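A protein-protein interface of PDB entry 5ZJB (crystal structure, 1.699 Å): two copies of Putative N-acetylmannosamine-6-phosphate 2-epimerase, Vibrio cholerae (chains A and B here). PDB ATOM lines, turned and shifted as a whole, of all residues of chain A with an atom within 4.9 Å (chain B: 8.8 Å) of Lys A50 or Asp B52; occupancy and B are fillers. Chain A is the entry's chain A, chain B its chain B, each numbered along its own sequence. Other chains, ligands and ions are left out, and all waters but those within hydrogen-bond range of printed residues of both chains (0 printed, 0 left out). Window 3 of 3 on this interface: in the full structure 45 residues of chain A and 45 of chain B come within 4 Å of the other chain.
The side-chain amino group (NZ) of Lys A50 is in salt-bridge range of the side-chain carboxylate (OD2) of Asp B52, at 3.6 Å.
NZ of Lys B50 lies within salt-bridge range of OD2 of Asp B52 (3.5 Å).
O of Ala B56 touches CG of Pro A47, 3.5 Å away.
Ile B59 touches Pro A47.
Ala B56 touches Leu A48 (CB to CD2, 3.5 Å).
N of Met B57 touches CD2 of Leu A48, 3.8 Å away.
CZ of Phe B53 touches O of Asp A52, 3.9 Å away.
CE1 of Phe A53 touches CD2 of Leu B48, 3.8 Å away.
CD1 of Phe A53 touches CD1 of Phe B53, 3.6 Å away.
Printed residues of chain B within 4 Å of Pro A47: Ala B56 (3.5 Å) and Ile B59 (3.7 Å).
Lys A50 touches one residue of chain B.
Printed residues of chain B within 4 Å of Phe A53: Leu B48 and Phe B53.
Of the printed residues of chain A, Leu B48 touches Phe A53.
Asp B49 touches none of the printed residues of chain A.
Of the printed residues of chain A, Asp B52 touches Lys A50.
Of the printed residues of chain A, Ala B56 touches Pro A47 (3.5 Å) and Leu A48 (3.5 Å).
Of the printed residues of chain A, Ile B59 touches Pro A47.
Ser B75 touches none of the printed residues of chain A.
The nearest printed residue of chain A that does not touch Asp B52 is Asp A52 (6.0 Å).
Printed residues of chain B that touch a printed residue of chain A: Leu B48, Asp B52, Phe B53, Ala B56, Met B57 and Ile B59.
Hydrophobic or aromatic side chains of chain B within 4 Å of the printed part of chain A: Leu B48, Phe B53, Ala B56, Met B57 and Ile B59.
Hydrophobic or aromatic side chains of chain A that line the printed part of chain B: Pro A47, Leu A48 and Phe A53.
Among the printed residues, 8 pairs touch across the chains.
Lys A50 touches Asp B52, but with the chains exchanged Asp A52 does not touch Lys B50 (5.6 Å).
Asp A52 touches Phe B53, but with the chains exchanged Phe A53 does not touch Asp B52 (6.8 Å).
Phe A53 touches Leu B48, but with the chains exchanged Leu A48 does not touch Phe B53 (4.7 Å).
Phe B53 touches its own counterpart, Phe A53.
Positions printed for both chains: 47, 48, 49, 50, 51, 52, 53 and 54.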
ATOM      1  N   PRO A  47      34.350   2.626   1.658  1.00  0.00           N
ATOM      2  CA  PRO A  47      33.370   2.751   2.744  1.00  0.00           C
ATOM      3  C   PRO A  47      31.983   3.088   2.236  1.00  0.00           C
ATOM      4  O   PRO A  47      30.999   2.826   2.938  1.00  0.00           O
ATOM      5  CB  PRO A  47      33.944   3.878   3.629  1.00  0.00           C
ATOM      6  CG  PRO A  47      34.961   4.577   2.764  1.00  0.00           C
ATOM      7  CD  PRO A  47      35.481   3.565   1.793  1.00  0.00           C
ATOM      8  N   LEU A  48      31.874   3.639   1.023  1.00  0.00           N
ATOM      9  CA  LEU A  48      30.586   4.010   0.461  1.00  0.00           C
ATOM     10  C   LEU A  48      29.858   2.831  -0.161  1.00  0.00           C
ATOM     11  O   LEU A  48      28.669   2.958  -0.474  1.00  0.00           O
ATOM     12  CB  LEU A  48      30.777   5.110  -0.585  1.00  0.00           C
ATOM     13  CG  LEU A  48      31.490   6.323   0.021  1.00  0.00           C
ATOM     14  CD1 LEU A  48      31.771   7.318  -1.087  1.00  0.00           C
ATOM     15  CD2 LEU A  48      30.606   6.907   1.095  1.00  0.00           C
ATOM     16  N   ASP A  49      30.537   1.699  -0.361  1.00  0.00           N
ATOM     17  CA  ASP A  49      29.909   0.539  -1.008  1.00  0.00           C
ATOM     18  C   ASP A  49      29.212  -0.272   0.075  1.00  0.00           C
ATOM     19  O   ASP A  49      29.688  -1.316   0.533  1.00  0.00           O
ATOM     20  CB  ASP A  49      30.938  -0.288  -1.760  1.00  0.00           C
ATOM     21  CG  ASP A  49      30.305  -1.446  -2.502  1.00  0.00           C
ATOM     22  OD1 ASP A  49      29.082  -1.364  -2.769  1.00  0.00           O
ATOM     23  OD2 ASP A  49      31.022  -2.417  -2.810  1.00  0.00           O
ATOM     24  N   LYS A  50      28.065   0.241   0.498  1.00  0.00           N
ATOM     25  CA  LYS A  50      27.305  -0.303   1.611  1.00  0.00           C
ATOM     26  C   LYS A  50      25.830  -0.189   1.257  1.00  0.00           C
ATOM     27  O   LYS A  50      25.396   0.825   0.711  1.00  0.00           O
ATOM     28  CB  LYS A  50      27.644   0.463   2.909  1.00  0.00           C
ATOM     29  CG  LYS A  50      26.720   0.269   4.097  1.00  0.00           C
ATOM     30  CD  LYS A  50      27.118   1.249   5.229  1.00  0.00           C
ATOM     31  CE  LYS A  50      26.246   1.080   6.468  1.00  0.00           C
ATOM     32  NZ  LYS A  50      26.684   1.965   7.585  1.00  0.00           N
ATOM     33  N   THR A  51      25.054  -1.243   1.534  1.00  0.00           N
ATOM     34  CA  THR A  51      23.658  -1.198   1.112  1.00  0.00           C
ATOM     35  C   THR A  51      22.929   0.010   1.702  1.00  0.00           C
ATOM     36  O   THR A  51      22.138   0.659   1.008  1.00  0.00           O
ATOM     37  CB  THR A  51      22.947  -2.504   1.477  1.00  0.00           C
ATOM     38  OG1 THR A  51      23.590  -3.581   0.786  1.00  0.00           O
ATOM     39  CG2 THR A  51      21.473  -2.455   1.034  1.00  0.00           C
ATOM     40  N   ASP A  52      23.196   0.347   2.972  1.00  0.00           N
ATOM     41  CA  ASP A  52      22.525   1.498   3.578  1.00  0.00           C
ATOM     42  C   ASP A  52      22.808   2.784   2.806  1.00  0.00           C
ATOM     43  O   ASP A  52      21.918   3.626   2.642  1.00  0.00           O
ATOM     44  CB  ASP A  52      22.943   1.672   5.040  1.00  0.00           C
ATOM     45  CG  ASP A  52      22.325   0.634   5.969  1.00  0.00           C
ATOM     46  OD1 ASP A  52      21.415  -0.107   5.544  1.00  0.00           O
ATOM     47  OD2 ASP A  52      22.746   0.578   7.147  1.00  0.00           O
ATOM     48  N   PHE A  53      24.046   2.966   2.342  1.00  0.00           N
ATOM     49  CA  PHE A  53      24.395   4.182   1.600  1.00  0.00           C
ATOM     50  C   PHE A  53      23.809   4.158   0.193  1.00  0.00           C
ATOM     51  O   PHE A  53      23.404   5.197  -0.337  1.00  0.00           O
ATOM     52  CB  PHE A  53      25.920   4.349   1.550  1.00  0.00           C
ATOM     53  CG  PHE A  53      26.391   5.669   0.958  1.00  0.00           C
ATOM     54  CD1 PHE A  53      26.163   6.868   1.623  1.00  0.00           C
ATOM     55  CD2 PHE A  53      27.096   5.702  -0.237  1.00  0.00           C
ATOM     56  CE1 PHE A  53      26.606   8.080   1.093  1.00  0.00           C
ATOM     57  CE2 PHE A  53      27.539   6.912  -0.774  1.00  0.00           C
ATOM     58  CZ  PHE A  53      27.295   8.103  -0.100  1.00  0.00           C
ATOM     59  N   ILE A  54      23.768   2.987  -0.437  1.00  0.00           N
ATOM     60  CA  ILE A  54      23.152   2.888  -1.755  1.00  0.00           C
ATOM     61  C   ILE A  54      21.674   3.235  -1.667  1.00  0.00           C
ATOM     62  O   ILE A  54      21.143   3.983  -2.502  1.00  0.00           O
ATOM     63  CB  ILE A  54      23.383   1.480  -2.331  1.00  0.00           C
ATOM     64  CG1 ILE A  54      24.864   1.306  -2.672  1.00  0.00           C
ATOM     65  CG2 ILE A  54      22.515   1.266  -3.555  1.00  0.00           C
ATOM     66  CD1 ILE A  54      25.298  -0.141  -2.879  1.00  0.00           C
ATOM     67  N   ILE B  40      32.523  18.628   2.552  1.00  0.00           N
ATOM     68  CA  ILE B  40      31.552  17.545   2.674  1.00  0.00           C
ATOM     69  C   ILE B  40      30.364  18.054   3.471  1.00  0.00           C
ATOM     70  O   ILE B  40      30.283  17.864   4.694  1.00  0.00           O
ATOM     71  CB  ILE B  40      32.194  16.308   3.312  1.00  0.00           C
ATOM     72  CG1 ILE B  40      33.457  15.938   2.541  1.00  0.00           C
ATOM     73  CG2 ILE B  40      31.208  15.118   3.306  1.00  0.00           C
ATOM     74  CD1 ILE B  40      34.137  14.687   3.091  1.00  0.00           C
ATOM     75  N   PRO B  42      26.472  17.699   2.980  1.00  0.00           N
ATOM     76  CA  PRO B  42      25.308  17.202   2.231  1.00  0.00           C
ATOM     77  C   PRO B  42      24.134  18.168   2.314  1.00  0.00           C
ATOM     78  O   PRO B  42      24.070  19.053   3.170  1.00  0.00           O
ATOM     79  CB  PRO B  42      24.969  15.874   2.929  1.00  0.00           C
ATOM     80  CG  PRO B  42      26.199  15.498   3.713  1.00  0.00           C
ATOM     81  CD  PRO B  42      26.903  16.781   4.048  1.00  0.00           C
ATOM     82  N   PRO B  47      18.665  12.223   3.214  1.00  0.00           N
ATOM     83  CA  PRO B  47      19.058  10.954   3.843  1.00  0.00           C
ATOM     84  C   PRO B  47      20.565  10.780   3.897  1.00  0.00           C
ATOM     85  O   PRO B  47      21.053   9.937   4.661  1.00  0.00           O
ATOM     86  CB  PRO B  47      18.389   9.888   2.952  1.00  0.00           C
ATOM     87  CG  PRO B  47      18.093  10.562   1.682  1.00  0.00           C
ATOM     88  CD  PRO B  47      17.870  12.023   1.989  1.00  0.00           C
ATOM     89  N   LEU B  48      21.312  11.561   3.103  1.00  0.00           N
ATOM     90  CA  LEU B  48      22.766  11.547   3.089  1.00  0.00           C
ATOM     91  C   LEU B  48      23.362  12.464   4.143  1.00  0.00           C
ATOM     92  O   LEU B  48      24.567  12.385   4.401  1.00  0.00           O
ATOM     93  CB  LEU B  48      23.291  11.970   1.705  1.00  0.00           C
ATOM     94  CG  LEU B  48      22.736  11.131   0.543  1.00  0.00           C
ATOM     95  CD1 LEU B  48      23.115  11.716  -0.799  1.00  0.00           C
ATOM     96  CD2 LEU B  48      23.237   9.690   0.657  1.00  0.00           C
ATOM     97  N   ASP B  49      22.550  13.322   4.757  1.00  0.00           N
ATOM     98  CA  ASP B  49      23.036  14.276   5.756  1.00  0.00           C
ATOM     99  C   ASP B  49      23.074  13.591   7.124  1.00  0.00           C
ATOM    100  O   ASP B  49      22.286  13.876   8.029  1.00  0.00           O
ATOM    101  CB  ASP B  49      22.157  15.516   5.767  1.00  0.00           C
ATOM    102  CG  ASP B  49      22.716  16.612   6.642  1.00  0.00           C
ATOM    103  OD1 ASP B  49      23.931  16.572   6.942  1.00  0.00           O
ATOM    104  OD2 ASP B  49      21.939  17.502   7.027  1.00  0.00           O
ATOM    105  N   LYS B  50      24.031  12.667   7.251  1.00  0.00           N
ATOM    106  CA  LYS B  50      24.171  11.782   8.396  1.00  0.00           C
ATOM    107  C   LYS B  50      25.649  11.648   8.737  1.00  0.00           C
ATOM    108  O   LYS B  50      26.479  11.461   7.845  1.00  0.00           O
ATOM    109  CB  LYS B  50      23.569  10.399   8.069  1.00  0.00           C
ATOM    110  CG  LYS B  50      23.201   9.542   9.248  1.00  0.00           C
ATOM    111  CD  LYS B  50      22.591   8.225   8.763  1.00  0.00           C
ATOM    112  CE  LYS B  50      22.629   7.168   9.856  1.00  0.00           C
ATOM    113  NZ  LYS B  50      22.574   5.789   9.290  1.00  0.00           N
ATOM    114  N   THR B  51      25.976  11.715  10.030  1.00  0.00           N
ATOM    115  CA  THR B  51      27.379  11.675  10.436  1.00  0.00           C
ATOM    116  C   THR B  51      28.121  10.461   9.872  1.00  0.00           C
ATOM    117  O   THR B  51      29.262  10.589   9.407  1.00  0.00           O
ATOM    118  CB  THR B  51      27.486  11.715  11.961  1.00  0.00           C
ATOM    119  OG1 THR B  51      27.105  13.022  12.416  1.00  0.00           O
ATOM    120  CG2 THR B  51      28.916  11.454  12.389  1.00  0.00           C
ATOM    121  N   ASP B  52      27.513   9.267   9.915  1.00  0.00           N
ATOM    122  CA  ASP B  52      28.254   8.105   9.440  1.00  0.00           C
ATOM    123  C   ASP B  52      28.502   8.163   7.936  1.00  0.00           C
ATOM    124  O   ASP B  52      29.521   7.646   7.463  1.00  0.00           O
ATOM    125  CB  ASP B  52      27.549   6.804   9.838  1.00  0.00           C
ATOM    126  CG  ASP B  52      26.373   6.466   8.951  1.00  0.00           C
ATOM    127  OD1 ASP B  52      25.783   7.380   8.343  1.00  0.00           O
ATOM    128  OD2 ASP B  52      26.028   5.266   8.880  1.00  0.00           O
ATOM    129  N   PHE B  53      27.604   8.787   7.165  1.00  0.00           N
ATOM    130  CA  PHE B  53      27.844   8.954   5.737  1.00  0.00           C
ATOM    131  C   PHE B  53      28.874  10.044   5.475  1.00  0.00           C
ATOM    132  O   PHE B  53      29.701   9.914   4.569  1.00  0.00           O
ATOM    133  CB  PHE B  53      26.534   9.274   5.016  1.00  0.00           C
ATOM    134  CG  PHE B  53      25.541   8.147   5.039  1.00  0.00           C
ATOM    135  CD1 PHE B  53      25.964   6.837   5.168  1.00  0.00           C
ATOM    136  CD2 PHE B  53      24.189   8.401   4.930  1.00  0.00           C
ATOM    137  CE1 PHE B  53      25.049   5.796   5.184  1.00  0.00           C
ATOM    138  CE2 PHE B  53      23.272   7.374   4.948  1.00  0.00           C
ATOM    139  CZ  PHE B  53      23.700   6.068   5.076  1.00  0.00           C
ATOM    140  N   ILE B  54      28.837  11.120   6.260  1.00  0.00           N
ATOM    141  CA  ILE B  54      29.849  12.162   6.108  1.00  0.00           C
ATOM    142  C   ILE B  54      31.237  11.599   6.397  1.00  0.00           C
ATOM    143  O   ILE B  54      32.195  11.877   5.664  1.00  0.00           O
ATOM    144  CB  ILE B  54      29.505  13.364   7.000  1.00  0.00           C
ATOM    145  CG1 ILE B  54      28.327  14.124   6.378  1.00  0.00           C
ATOM    146  CG2 ILE B  54      30.732  14.289   7.150  1.00  0.00           C
ATOM    147  CD1 ILE B  54      27.667  15.124   7.301  1.00  0.00           C
ATOM    148  N   VAL B  55      31.356  10.753   7.435  1.00  0.00           N
ATOM    149  CA  VAL B  55      32.619  10.070   7.727  1.00  0.00           C
ATOM    150  C   VAL B  55      33.011   9.154   6.571  1.00  0.00           C
ATOM    151  O   VAL B  55      34.162   9.142   6.127  1.00  0.00           O
ATOM    152  CB  VAL B  55      32.521   9.292   9.056  1.00  0.00           C
ATOM    153  CG1 VAL B  55      33.762   8.411   9.246  1.00  0.00           C
ATOM    154  CG2 VAL B  55      32.360  10.249  10.244  1.00  0.00           C
ATOM    155  N   ALA B  56      32.063   8.362   6.064  1.00  0.00           N
ATOM    156  CA  ALA B  56      32.398   7.489   4.940  1.00  0.00           C
ATOM    157  C   ALA B  56      32.912   8.281   3.740  1.00  0.00           C
ATOM    158  O   ALA B  56      33.853   7.851   3.066  1.00  0.00           O
ATOM    159  CB  ALA B  56      31.184   6.639   4.539  1.00  0.00           C
ATOM    160  N   MET B  57      32.288   9.423   3.433  1.00  0.00           N
ATOM    161  CA  MET B  57      32.757  10.226   2.313  1.00  0.00           C
ATOM    162  C   MET B  57      34.141  10.795   2.596  1.00  0.00           C
ATOM    163  O   MET B  57      34.974  10.878   1.685  1.00  0.00           O
ATOM    164  CB  MET B  57      31.771  11.357   2.007  1.00  0.00           C
ATOM    165  CG  MET B  57      30.462  10.887   1.334  1.00  0.00           C
ATOM    166  SD  MET B  57      29.563  12.298   0.628  1.00  0.00           S
ATOM    167  CE  MET B  57      28.588  12.745   2.045  1.00  0.00           C
ATOM    168  N   ALA B  58      34.389  11.209   3.839  1.00  0.00           N
ATOM    169  CA  ALA B  58      35.701  11.756   4.181  1.00  0.00           C
ATOM    170  C   ALA B  58      36.782  10.701   4.006  1.00  0.00           C
ATOM    171  O   ALA B  58      37.853  10.966   3.446  1.00  0.00           O
ATOM    172  CB  ALA B  58      35.693  12.289   5.616  1.00  0.00           C
ATOM    173  N   ILE B  59      36.522   9.488   4.493  1.00  0.00           N
ATOM    174  CA  ILE B  59      37.468   8.401   4.293  1.00  0.00           C
ATOM    175  C   ILE B  59      37.666   8.146   2.803  1.00  0.00           C
ATOM    176  O   ILE B  59      38.793   7.984   2.323  1.00  0.00           O
ATOM    177  CB  ILE B  59      36.985   7.129   5.016  1.00  0.00           C
ATOM    178  CG1 ILE B  59      36.935   7.325   6.537  1.00  0.00           C
ATOM    179  CG2 ILE B  59      37.871   5.934   4.628  1.00  0.00           C
ATOM    180  CD1 ILE B  59      36.113   6.221   7.237  1.00  0.00           C
ATOM    181  N   SER B  75      30.353  18.011  16.002  1.00  0.00           N
ATOM    182  CA  SER B  75      30.313  16.554  16.086  1.00  0.00           C
ATOM    183  C   SER B  75      30.868  15.911  14.817  1.00  0.00           C
ATOM    184  O   SER B  75      31.578  14.893  14.882  1.00  0.00           O
ATOM    185  CB  SER B  75      28.879  16.082  16.354  1.00  0.00           C
ATOM    186  OG  SER B  75      28.471  16.468  17.657  1.00  0.00           O
ATOM    187  N   ASN B  76      30.559  16.491  13.653  1.00  0.00           N
ATOM    188  CA  ASN B  76      31.094  15.971  12.392  1.00  0.00           C
ATOM    189  C   ASN B  76      32.607  16.147  12.332  1.00  0.00           C
ATOM    190  O   ASN B  76      33.325  15.239  11.908  1.00  0.00           O
ATOM    191  CB  ASN B  76      30.428  16.665  11.200  1.00  0.00           C
ATOM    192  CG  ASN B  76      28.994  16.208  10.972  1.00  0.00           C
ATOM    193  OD1 ASN B  76      28.636  15.064  11.272  1.00  0.00           O
ATOM    194  ND2 ASN B  76      28.171  17.098  10.429  1.00  0.00           N
ATOM    195  N   ALA B  79      34.103  13.440  14.478  1.00  0.00           N
ATOM    196  CA  ALA B  79      34.012  12.095  13.909  1.00  0.00           C
ATOM    197  C   ALA B  79      34.945  11.938  12.715  1.00  0.00           C
ATOM    198  O   ALA B  79      35.577  10.884  12.537  1.00  0.00           O
ATOM    199  CB  ALA B  79      32.566  11.802  13.503  1.00  0.00           C
ATOM    200  N   VAL B  80      35.048  12.974  11.884  1.00  0.00           N
ATOM    201  CA  VAL B  80      35.910  12.884  10.715  1.00  0.00           C
ATOM    202  C   VAL B  80      37.376  12.881  11.120  1.00  0.00           C
ATOM    203  O   VAL B  80      38.182  12.133  10.556  1.00  0.00           O
ATOM    204  CB  VAL B  80      35.593  14.021   9.733  1.00  0.00           C
ATOM    205  CG1 VAL B  80      36.661  14.083   8.661  1.00  0.00           C
ATOM    206  CG2 VAL B  80      34.205  13.782   9.099  1.00  0.00           C
ATOM    207  N   ALA B  83      38.683   9.627  11.969  1.00  0.00           N
ATOM    208  CA  ALA B  83      38.683   8.618  10.914  1.00  0.00           C
ATOM    209  C   ALA B  83      39.745   8.844   9.847  1.00  0.00           C
ATOM    210  O   ALA B  83      40.107   7.882   9.160  1.00  0.00           O
ATOM    211  CB  ALA B  83      37.310   8.557  10.231  1.00  0.00           C
